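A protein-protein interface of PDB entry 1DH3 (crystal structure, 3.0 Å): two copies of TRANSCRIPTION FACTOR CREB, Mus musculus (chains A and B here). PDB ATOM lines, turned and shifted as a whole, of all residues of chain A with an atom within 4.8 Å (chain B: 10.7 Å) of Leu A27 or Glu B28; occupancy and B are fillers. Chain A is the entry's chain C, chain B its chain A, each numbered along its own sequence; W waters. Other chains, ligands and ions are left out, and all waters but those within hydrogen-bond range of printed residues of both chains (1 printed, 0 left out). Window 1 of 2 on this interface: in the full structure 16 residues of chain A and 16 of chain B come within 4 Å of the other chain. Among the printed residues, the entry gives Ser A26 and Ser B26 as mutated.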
ATOM      1  N   TYR A  23     -17.044 -11.783   3.256  1.00  0.00           N
ATOM      2  CA  TYR A  23     -16.435 -10.839   4.158  1.00  0.00           C
ATOM      3  C   TYR A  23     -14.935 -10.827   4.117  1.00  0.00           C
ATOM      4  O   TYR A  23     -14.269 -10.025   4.726  1.00  0.00           O
ATOM      5  CB  TYR A  23     -17.059 -11.004   5.517  1.00  0.00           C
ATOM      6  CG  TYR A  23     -16.245 -10.526   6.662  1.00  0.00           C
ATOM      7  CD1 TYR A  23     -16.640  -9.423   7.321  1.00  0.00           C
ATOM      8  CD2 TYR A  23     -15.145 -11.185   7.108  1.00  0.00           C
ATOM      9  CE1 TYR A  23     -15.993  -8.985   8.410  1.00  0.00           C
ATOM     10  CE2 TYR A  23     -14.444 -10.727   8.170  1.00  0.00           C
ATOM     11  CZ  TYR A  23     -14.872  -9.619   8.818  1.00  0.00           C
ATOM     12  OH  TYR A  23     -14.212  -9.145   9.914  1.00  0.00           O
ATOM     13  N   VAL A  24     -14.314 -11.690   3.378  1.00  0.00           N
ATOM     14  CA  VAL A  24     -12.943 -11.399   3.559  1.00  0.00           C
ATOM     15  C   VAL A  24     -12.593 -10.608   2.360  1.00  0.00           C
ATOM     16  O   VAL A  24     -11.744  -9.706   2.397  1.00  0.00           O
ATOM     17  CB  VAL A  24     -12.072 -12.472   4.004  1.00  0.00           C
ATOM     18  CG1 VAL A  24     -12.552 -13.697   3.481  1.00  0.00           C
ATOM     19  CG2 VAL A  24     -10.820 -12.235   3.404  1.00  0.00           C
ATOM     20  N   LYS A  25     -13.291 -10.923   1.285  1.00  0.00           N
ATOM     21  CA  LYS A  25     -13.066 -10.193   0.014  1.00  0.00           C
ATOM     22  C   LYS A  25     -13.152  -8.676   0.226  1.00  0.00           C
ATOM     23  O   LYS A  25     -12.236  -7.885   0.014  1.00  0.00           O
ATOM     24  CB  LYS A  25     -14.170 -10.558  -0.985  1.00  0.00           C
ATOM     25  CG  LYS A  25     -14.005  -9.964  -2.404  1.00  0.00           C
ATOM     26  CD  LYS A  25     -13.459 -10.964  -3.497  1.00  0.00           C
ATOM     27  CE  LYS A  25     -13.599 -12.497  -3.163  1.00  0.00           C
ATOM     28  NZ  LYS A  25     -14.570 -13.299  -4.067  1.00  0.00           N
ATOM     29  N   SER A  26     -14.338  -8.353   0.667  1.00  0.00           N
ATOM     30  CA  SER A  26     -14.787  -7.055   0.999  1.00  0.00           C
ATOM     31  C   SER A  26     -13.680  -6.367   1.800  1.00  0.00           C
ATOM     32  O   SER A  26     -13.282  -5.223   1.468  1.00  0.00           O
ATOM     33  CB  SER A  26     -15.809  -7.364   2.050  1.00  0.00           C
ATOM     34  OG  SER A  26     -15.177  -8.356   2.867  1.00  0.00           O
ATOM     35  N   LEU A  27     -13.197  -7.068   2.827  1.00  0.00           N
ATOM     36  CA  LEU A  27     -12.177  -6.489   3.642  1.00  0.00           C
ATOM     37  C   LEU A  27     -11.002  -6.192   2.697  1.00  0.00           C
ATOM     38  O   LEU A  27     -10.452  -5.052   2.653  1.00  0.00           O
ATOM     39  CB  LEU A  27     -11.791  -7.410   4.810  1.00  0.00           C
ATOM     40  CG  LEU A  27     -12.328  -7.580   6.267  1.00  0.00           C
ATOM     41  CD1 LEU A  27     -11.264  -7.469   7.384  1.00  0.00           C
ATOM     42  CD2 LEU A  27     -13.715  -7.117   6.754  1.00  0.00           C
ATOM     43  N   GLU A  28     -10.674  -7.214   1.918  1.00  0.00           N
ATOM     44  CA  GLU A  28      -9.576  -7.078   0.998  1.00  0.00           C
ATOM     45  C   GLU A  28      -9.820  -5.900   0.140  1.00  0.00           C
ATOM     46  O   GLU A  28      -8.867  -5.382  -0.338  1.00  0.00           O
ATOM     47  CB  GLU A  28      -9.394  -8.285   0.072  1.00  0.00           C
ATOM     48  CG  GLU A  28      -9.219  -9.687   0.588  1.00  0.00           C
ATOM     49  CD  GLU A  28      -8.268 -10.456  -0.308  1.00  0.00           C
ATOM     50  OE1 GLU A  28      -8.265 -10.181  -1.523  1.00  0.00           O
ATOM     51  OE2 GLU A  28      -7.508 -11.304   0.207  1.00  0.00           O
ATOM     52  N   ASN A  29     -11.062  -5.471  -0.040  1.00  0.00           N
ATOM     53  CA  ASN A  29     -11.192  -4.311  -0.896  1.00  0.00           C
ATOM     54  C   ASN A  29     -10.734  -3.141  -0.069  1.00  0.00           C
ATOM     55  O   ASN A  29      -9.637  -2.648  -0.202  1.00  0.00           O
ATOM     56  CB  ASN A  29     -12.620  -3.943  -1.292  1.00  0.00           C
ATOM     57  CG  ASN A  29     -13.232  -4.925  -2.291  1.00  0.00           C
ATOM     58  OD1 ASN A  29     -12.717  -6.047  -2.460  1.00  0.00           O
ATOM     59  ND2 ASN A  29     -14.382  -4.533  -2.897  1.00  0.00           N
ATOM     60  N   ARG A  30     -11.642  -2.743   0.789  1.00  0.00           N
ATOM     61  CA  ARG A  30     -11.552  -1.676   1.711  1.00  0.00           C
ATOM     62  C   ARG A  30     -10.254  -1.086   1.949  1.00  0.00           C
ATOM     63  O   ARG A  30      -9.993   0.103   1.805  1.00  0.00           O
ATOM     64  CB  ARG A  30     -11.912  -2.218   3.036  1.00  0.00           C
ATOM     65  CG  ARG A  30     -12.213  -1.099   3.997  1.00  0.00           C
ATOM     66  CD  ARG A  30     -13.733  -1.080   4.335  1.00  0.00           C
ATOM     67  NE  ARG A  30     -14.077   0.086   5.150  1.00  0.00           N
ATOM     68  CZ  ARG A  30     -14.532   1.230   4.630  1.00  0.00           C
ATOM     69  NH1 ARG A  30     -14.693   1.345   3.308  1.00  0.00           N
ATOM     70  NH2 ARG A  30     -14.828   2.269   5.418  1.00  0.00           N
ATOM     71  N   VAL A  31      -9.430  -2.010   2.316  1.00  0.00           N
ATOM     72  CA  VAL A  31      -8.052  -1.670   2.609  1.00  0.00           C
ATOM     73  C   VAL A  31      -7.470  -0.996   1.370  1.00  0.00           C
ATOM     74  O   VAL A  31      -6.815   0.007   1.498  1.00  0.00           O
ATOM     75  CB  VAL A  31      -7.270  -2.909   2.631  1.00  0.00           C
ATOM     76  CG1 VAL A  31      -7.126  -3.475   3.980  1.00  0.00           C
ATOM     77  CG2 VAL A  31      -8.104  -3.826   1.819  1.00  0.00           C
ATOM     78  N   LYS B  20      -4.996 -18.581   7.803  1.00  0.00           N
ATOM     79  CA  LYS B  20      -6.171 -17.867   7.320  1.00  0.00           C
ATOM     80  C   LYS B  20      -6.549 -16.963   8.382  1.00  0.00           C
ATOM     81  O   LYS B  20      -6.581 -15.802   8.165  1.00  0.00           O
ATOM     82  CB  LYS B  20      -7.389 -18.772   7.099  1.00  0.00           C
ATOM     83  CG  LYS B  20      -7.951 -18.814   5.666  1.00  0.00           C
ATOM     84  CD  LYS B  20      -9.323 -18.189   5.679  1.00  0.00           C
ATOM     85  CE  LYS B  20     -10.139 -18.428   4.422  1.00  0.00           C
ATOM     86  NZ  LYS B  20     -11.603 -18.234   4.810  1.00  0.00           N
ATOM     87  N   LYS B  21      -6.813 -17.563   9.519  1.00  0.00           N
ATOM     88  CA  LYS B  21      -7.254 -16.894  10.715  1.00  0.00           C
ATOM     89  C   LYS B  21      -6.631 -15.629  10.908  1.00  0.00           C
ATOM     90  O   LYS B  21      -7.293 -14.599  10.820  1.00  0.00           O
ATOM     91  CB  LYS B  21      -7.310 -17.769  11.990  1.00  0.00           C
ATOM     92  CG  LYS B  21      -7.999 -17.166  13.265  1.00  0.00           C
ATOM     93  CD  LYS B  21      -8.653 -18.204  14.326  1.00  0.00           C
ATOM     94  CE  LYS B  21      -9.924 -17.641  15.141  1.00  0.00           C
ATOM     95  NZ  LYS B  21      -9.844 -17.554  16.671  1.00  0.00           N
ATOM     96  N   GLU B  22      -5.353 -15.711  11.108  1.00  0.00           N
ATOM     97  CA  GLU B  22      -4.601 -14.516  11.312  1.00  0.00           C
ATOM     98  C   GLU B  22      -4.812 -13.531  10.222  1.00  0.00           C
ATOM     99  O   GLU B  22      -5.058 -12.356  10.509  1.00  0.00           O
ATOM    100  CB  GLU B  22      -3.107 -14.804  11.492  1.00  0.00           C
ATOM    101  CG  GLU B  22      -2.600 -14.553  12.940  1.00  0.00           C
ATOM    102  CD  GLU B  22      -1.544 -15.535  13.405  1.00  0.00           C
ATOM    103  OE1 GLU B  22      -0.352 -15.336  13.025  1.00  0.00           O
ATOM    104  OE2 GLU B  22      -1.899 -16.444  14.205  1.00  0.00           O
ATOM    105  N   TYR B  23      -4.734 -14.019   8.994  1.00  0.00           N
ATOM    106  CA  TYR B  23      -4.917 -13.147   7.849  1.00  0.00           C
ATOM    107  C   TYR B  23      -6.142 -12.288   7.960  1.00  0.00           C
ATOM    108  O   TYR B  23      -6.045 -11.059   7.753  1.00  0.00           O
ATOM    109  CB  TYR B  23      -5.155 -13.934   6.648  1.00  0.00           C
ATOM    110  CG  TYR B  23      -5.315 -13.133   5.413  1.00  0.00           C
ATOM    111  CD1 TYR B  23      -4.341 -12.325   4.944  1.00  0.00           C
ATOM    112  CD2 TYR B  23      -6.445 -13.337   4.626  1.00  0.00           C
ATOM    113  CE1 TYR B  23      -4.506 -11.578   3.777  1.00  0.00           C
ATOM    114  CE2 TYR B  23      -6.611 -12.727   3.410  1.00  0.00           C
ATOM    115  CZ  TYR B  23      -5.649 -11.776   3.010  1.00  0.00           C
ATOM    116  OH  TYR B  23      -5.760 -11.031   1.825  1.00  0.00           O
ATOM    117  N   VAL B  24      -7.273 -12.916   8.297  1.00  0.00           N
ATOM    118  CA  VAL B  24      -8.409 -12.077   8.393  1.00  0.00           C
ATOM    119  C   VAL B  24      -8.176 -11.188   9.506  1.00  0.00           C
ATOM    120  O   VAL B  24      -8.592 -10.022   9.372  1.00  0.00           O
ATOM    121  CB  VAL B  24      -9.712 -12.608   8.509  1.00  0.00           C
ATOM    122  CG1 VAL B  24      -9.715 -13.854   7.931  1.00  0.00           C
ATOM    123  CG2 VAL B  24     -10.041 -12.582   9.881  1.00  0.00           C
ATOM    124  N   LYS B  25      -7.492 -11.662  10.537  1.00  0.00           N
ATOM    125  CA  LYS B  25      -7.246 -10.679  11.605  1.00  0.00           C
ATOM    126  C   LYS B  25      -6.513  -9.480  11.059  1.00  0.00           C
ATOM    127  O   LYS B  25      -7.121  -8.410  11.048  1.00  0.00           O
ATOM    128  CB  LYS B  25      -6.714 -11.121  12.962  1.00  0.00           C
ATOM    129  CG  LYS B  25      -7.949 -10.995  13.991  1.00  0.00           C
ATOM    130  CD  LYS B  25      -8.054 -12.050  15.120  1.00  0.00           C
ATOM    131  CE  LYS B  25      -7.342 -11.617  16.430  1.00  0.00           C
ATOM    132  NZ  LYS B  25      -5.878 -12.053  16.598  1.00  0.00           N
ATOM    133  N   SER B  26      -5.304  -9.682  10.567  1.00  0.00           N
ATOM    134  CA  SER B  26      -4.453  -8.644   9.972  1.00  0.00           C
ATOM    135  C   SER B  26      -5.235  -7.607   9.206  1.00  0.00           C
ATOM    136  O   SER B  26      -5.087  -6.405   9.392  1.00  0.00           O
ATOM    137  CB  SER B  26      -3.496  -9.286   8.951  1.00  0.00           C
ATOM    138  OG  SER B  26      -3.526  -8.624   7.689  1.00  0.00           O
ATOM    139  N   LEU B  27      -6.116  -8.105   8.354  1.00  0.00           N
ATOM    140  CA  LEU B  27      -6.917  -7.223   7.555  1.00  0.00           C
ATOM    141  C   LEU B  27      -7.694  -6.400   8.435  1.00  0.00           C
ATOM    142  O   LEU B  27      -7.539  -5.223   8.367  1.00  0.00           O
ATOM    143  CB  LEU B  27      -7.914  -7.949   6.731  1.00  0.00           C
ATOM    144  CG  LEU B  27      -6.909  -8.671   5.878  1.00  0.00           C
ATOM    145  CD1 LEU B  27      -7.531  -9.877   5.136  1.00  0.00           C
ATOM    146  CD2 LEU B  27      -6.206  -7.642   5.022  1.00  0.00           C
ATOM    147  N   GLU B  28      -8.515  -7.038   9.256  1.00  0.00           N
ATOM    148  CA  GLU B  28      -9.385  -6.373  10.181  1.00  0.00           C
ATOM    149  C   GLU B  28      -8.588  -5.279  10.859  1.00  0.00           C
ATOM    150  O   GLU B  28      -9.069  -4.160  11.031  1.00  0.00           O
ATOM    151  CB  GLU B  28      -9.746  -7.391  11.216  1.00  0.00           C
ATOM    152  CG  GLU B  28     -10.780  -8.311  10.709  1.00  0.00           C
ATOM    153  CD  GLU B  28     -11.468  -9.110  11.788  1.00  0.00           C
ATOM    154  OE1 GLU B  28     -10.796  -9.559  12.767  1.00  0.00           O
ATOM    155  OE2 GLU B  28     -12.703  -9.222  11.630  1.00  0.00           O
ATOM    156  N   ASN B  29      -7.341  -5.551  11.179  1.00  0.00           N
ATOM    157  CA  ASN B  29      -6.605  -4.499  11.817  1.00  0.00           C
ATOM    158  C   ASN B  29      -6.292  -3.295  10.983  1.00  0.00           C
ATOM    159  O   ASN B  29      -6.910  -2.280  11.233  1.00  0.00           O
ATOM    160  CB  ASN B  29      -5.424  -4.985  12.568  1.00  0.00           C
ATOM    161  CG  ASN B  29      -4.989  -4.020  13.603  1.00  0.00           C
ATOM    162  OD1 ASN B  29      -5.173  -4.217  14.838  1.00  0.00           O
ATOM    163  ND2 ASN B  29      -4.370  -2.954  13.119  1.00  0.00           N
ATOM    164  N   ARG B  30      -5.374  -3.390  10.019  1.00  0.00           N
ATOM    165  CA  ARG B  30      -5.003  -2.252   9.137  1.00  0.00           C
ATOM    166  C   ARG B  30      -6.194  -1.538   8.672  1.00  0.00           C
ATOM    167  O   ARG B  30      -6.102  -0.392   8.395  1.00  0.00           O
ATOM    168  CB  ARG B  30      -4.157  -2.620   7.903  1.00  0.00           C
ATOM    169  CG  ARG B  30      -4.082  -4.089   7.646  1.00  0.00           C
ATOM    170  CD  ARG B  30      -2.891  -4.523   6.820  1.00  0.00           C
ATOM    171  NE  ARG B  30      -2.668  -3.632   5.700  1.00  0.00           N
ATOM    172  CZ  ARG B  30      -2.313  -3.974   4.461  1.00  0.00           C
ATOM    173  NH1 ARG B  30      -2.133  -5.234   4.115  1.00  0.00           N
ATOM    174  NH2 ARG B  30      -2.138  -3.043   3.551  1.00  0.00           N
ATOM    175  N   VAL B  31      -7.310  -2.230   8.614  1.00  0.00           N
ATOM    176  CA  VAL B  31      -8.517  -1.606   8.202  1.00  0.00           C
ATOM    177  C   VAL B  31      -8.764  -0.530   9.169  1.00  0.00           C
ATOM    178  O   VAL B  31      -9.278   0.522   8.851  1.00  0.00           O
ATOM    179  CB  VAL B  31      -9.773  -2.455   8.445  1.00  0.00           C
ATOM    180  CG1 VAL B  31     -10.674  -2.186   9.894  1.00  0.00           C
ATOM    181  CG2 VAL B  31     -10.612  -2.286   7.215  1.00  0.00           C
ATOM    182  N   ALA B  32      -8.385  -0.759  10.370  1.00  0.00           N
ATOM    183  CA  ALA B  32      -8.710   0.320  11.169  1.00  0.00           C
ATOM    184  C   ALA B  32      -7.545   1.174  11.323  1.00  0.00           C
ATOM    185  O   ALA B  32      -7.663   2.298  11.709  1.00  0.00           O
ATOM    186  CB  ALA B  32      -9.185  -0.219  12.512  1.00  0.00           C
ATOM    187  N   VAL B  33      -6.394   0.631  11.047  1.00  0.00           N
ATOM    188  CA  VAL B  33      -5.231   1.471  11.235  1.00  0.00           C
ATOM    189  C   VAL B  33      -5.359   2.557  10.221  1.00  0.00           C
ATOM    190  O   VAL B  33      -5.080   3.688  10.405  1.00  0.00           O
ATOM    191  CB  VAL B  33      -3.945   0.649  10.957  1.00  0.00           C
ATOM    192  CG1 VAL B  33      -3.602   0.541   9.433  1.00  0.00           C
ATOM    193  CG2 VAL B  33      -2.821   1.245  11.672  1.00  0.00           C
ATOM    194  N   LEU B  34      -5.873   2.123   9.121  1.00  0.00           N
ATOM    195  CA  LEU B  34      -6.013   3.006   8.064  1.00  0.00           C
ATOM    196  C   LEU B  34      -7.001   3.996   8.354  1.00  0.00           C
ATOM    197  O   LEU B  34      -6.781   5.220   8.174  1.00  0.00           O
ATOM    198  CB  LEU B  34      -6.273   2.211   6.781  1.00  0.00           C
ATOM    199  CG  LEU B  34      -4.821   1.773   6.501  1.00  0.00           C
ATOM    200  CD1 LEU B  34      -4.375   0.580   5.728  1.00  0.00           C
ATOM    201  CD2 LEU B  34      -3.845   2.906   6.432  1.00  0.00           C
ATOM    202  N   GLU B  35      -8.096   3.434   8.818  1.00  0.00           N
ATOM    203  CA  GLU B  35      -9.260   4.225   9.161  1.00  0.00           C
ATOM    204  C   GLU B  35      -8.830   5.405  10.000  1.00  0.00           C
ATOM    205  O   GLU B  35      -9.370   6.515   9.916  1.00  0.00           O
ATOM    206  CB  GLU B  35     -10.383   3.343   9.758  1.00  0.00           C
ATOM    207  CG  GLU B  35     -11.550   3.340   8.800  1.00  0.00           C
ATOM    208  CD  GLU B  35     -12.697   2.326   9.056  1.00  0.00           C
ATOM    209  OE1 GLU B  35     -13.480   2.078   8.073  1.00  0.00           O
ATOM    210  OE2 GLU B  35     -12.858   1.829  10.218  1.00  0.00           O
ATOM    211  N   ASN B  36      -7.791   5.125  10.763  1.00  0.00           N
ATOM    212  CA  ASN B  36      -7.312   6.136  11.583  1.00  0.00           C
ATOM    213  C   ASN B  36      -6.517   7.235  11.067  1.00  0.00           C
ATOM    214  O   ASN B  36      -6.965   8.345  11.152  1.00  0.00           O
ATOM    215  CB  ASN B  36      -6.771   5.624  12.851  1.00  0.00           C
ATOM    216  CG  ASN B  36      -7.520   6.167  13.976  1.00  0.00           C
ATOM    217  OD1 ASN B  36      -8.720   5.850  14.124  1.00  0.00           O
ATOM    218  ND2 ASN B  36      -6.891   7.065  14.744  1.00  0.00           N
HETATM  219  O   HOH W   1     -14.285  -0.635   8.019  1.00  0.00           O
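The side-chain carboxylate (OE2) of Glu A28 lies close to the side-chain hydroxyl (OH) of Tyr B23.
The side-chain carboxylate of Glu B28 sits close to the side-chain hydroxyl of Tyr A23.
The guanidinium group (NH2) of Arg A30 lies within salt-bridge range of the side-chain carboxylate (OE1) of Glu B35 (3.0 Å).
The backbone carbonyl oxygen of Tyr A23 lies within hydrogen-bond range of the side-chain hydroxyl of Ser A26 (2.7 Å).
Among the printed residues, merely in contact across the chains: Leu A27 with Glu B28 (3.4 Å), Leu A27 with Leu B27 (3.4 Å) and Arg A30 with Val B31 (3.8 Å).
Tyr A23 touches one residue of chain B.
No residue of chain B comes within 4 Å of Val A24.
Of the printed residues of chain B, Glu A28 touches Tyr B23.
No residue of chain B comes within 4 Å of Asn A29.
No residue of chain B comes within 4 Å of Val A31.
Of the printed residues of chain A, Leu B27 touches Leu A27 (3.4 Å).
Of the printed residues of chain A, Glu B28 touches Tyr A23 (2.3 Å) and Leu A27 (3.4 Å).
Printed residues of chain A within 4 Å of Val B31: Arg A30 (3.8 Å).
Leu B34 touches none of the printed residues of chain A.
Of the printed residues of chain A, Glu B35 touches Arg A30.
The nearest residue of chain B that does not touch Leu A27 is Val B24 (4.2 Å).
The nearest printed residue of chain A that does not touch Glu B28 is Val A31 (6.5 Å).
Printed residues of chain A that touch a printed residue of chain B: Tyr A23, Leu A27, Glu A28 and Arg A30.
Hydrophobic or aromatic side chains of chain A within 4 Å of the printed part of chain B: Tyr A23 and Leu A27.
Of the 17 printed residues of chain B, 5 touch a printed residue of chain A.
Hydrophobic or aromatic side chains of chain B within 4 Å of the printed part of chain A: Tyr B23, Leu B27 and Val B31.
Among the printed residues, 6 pairs touch across the chains.
Among the printed residues, Asp or Glu carboxylates within 4 Å of a Lys or Arg side-chain nitrogen of the other chain: Arg A30 with Glu B35 (3.0 Å).
Tyr A23 touches Glu B28, and with the chains exchanged Glu A28 touches Tyr B23.
Leu A27 touches its own counterpart, Leu B27.
Leu A27 touches Glu B28, but with the chains exchanged Glu A28 does not touch Leu B27 (4.9 Å).
Arg A30 touches Val B31, but with the chains exchanged Val A31 does not touch Arg B30 (4.8 Å).
9 positions are printed for both chains.
Water W1 lies within hydrogen-bond range of OE1 of Glu B35 (2.8 Å) and NE of Arg A30 (3.0 Å).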
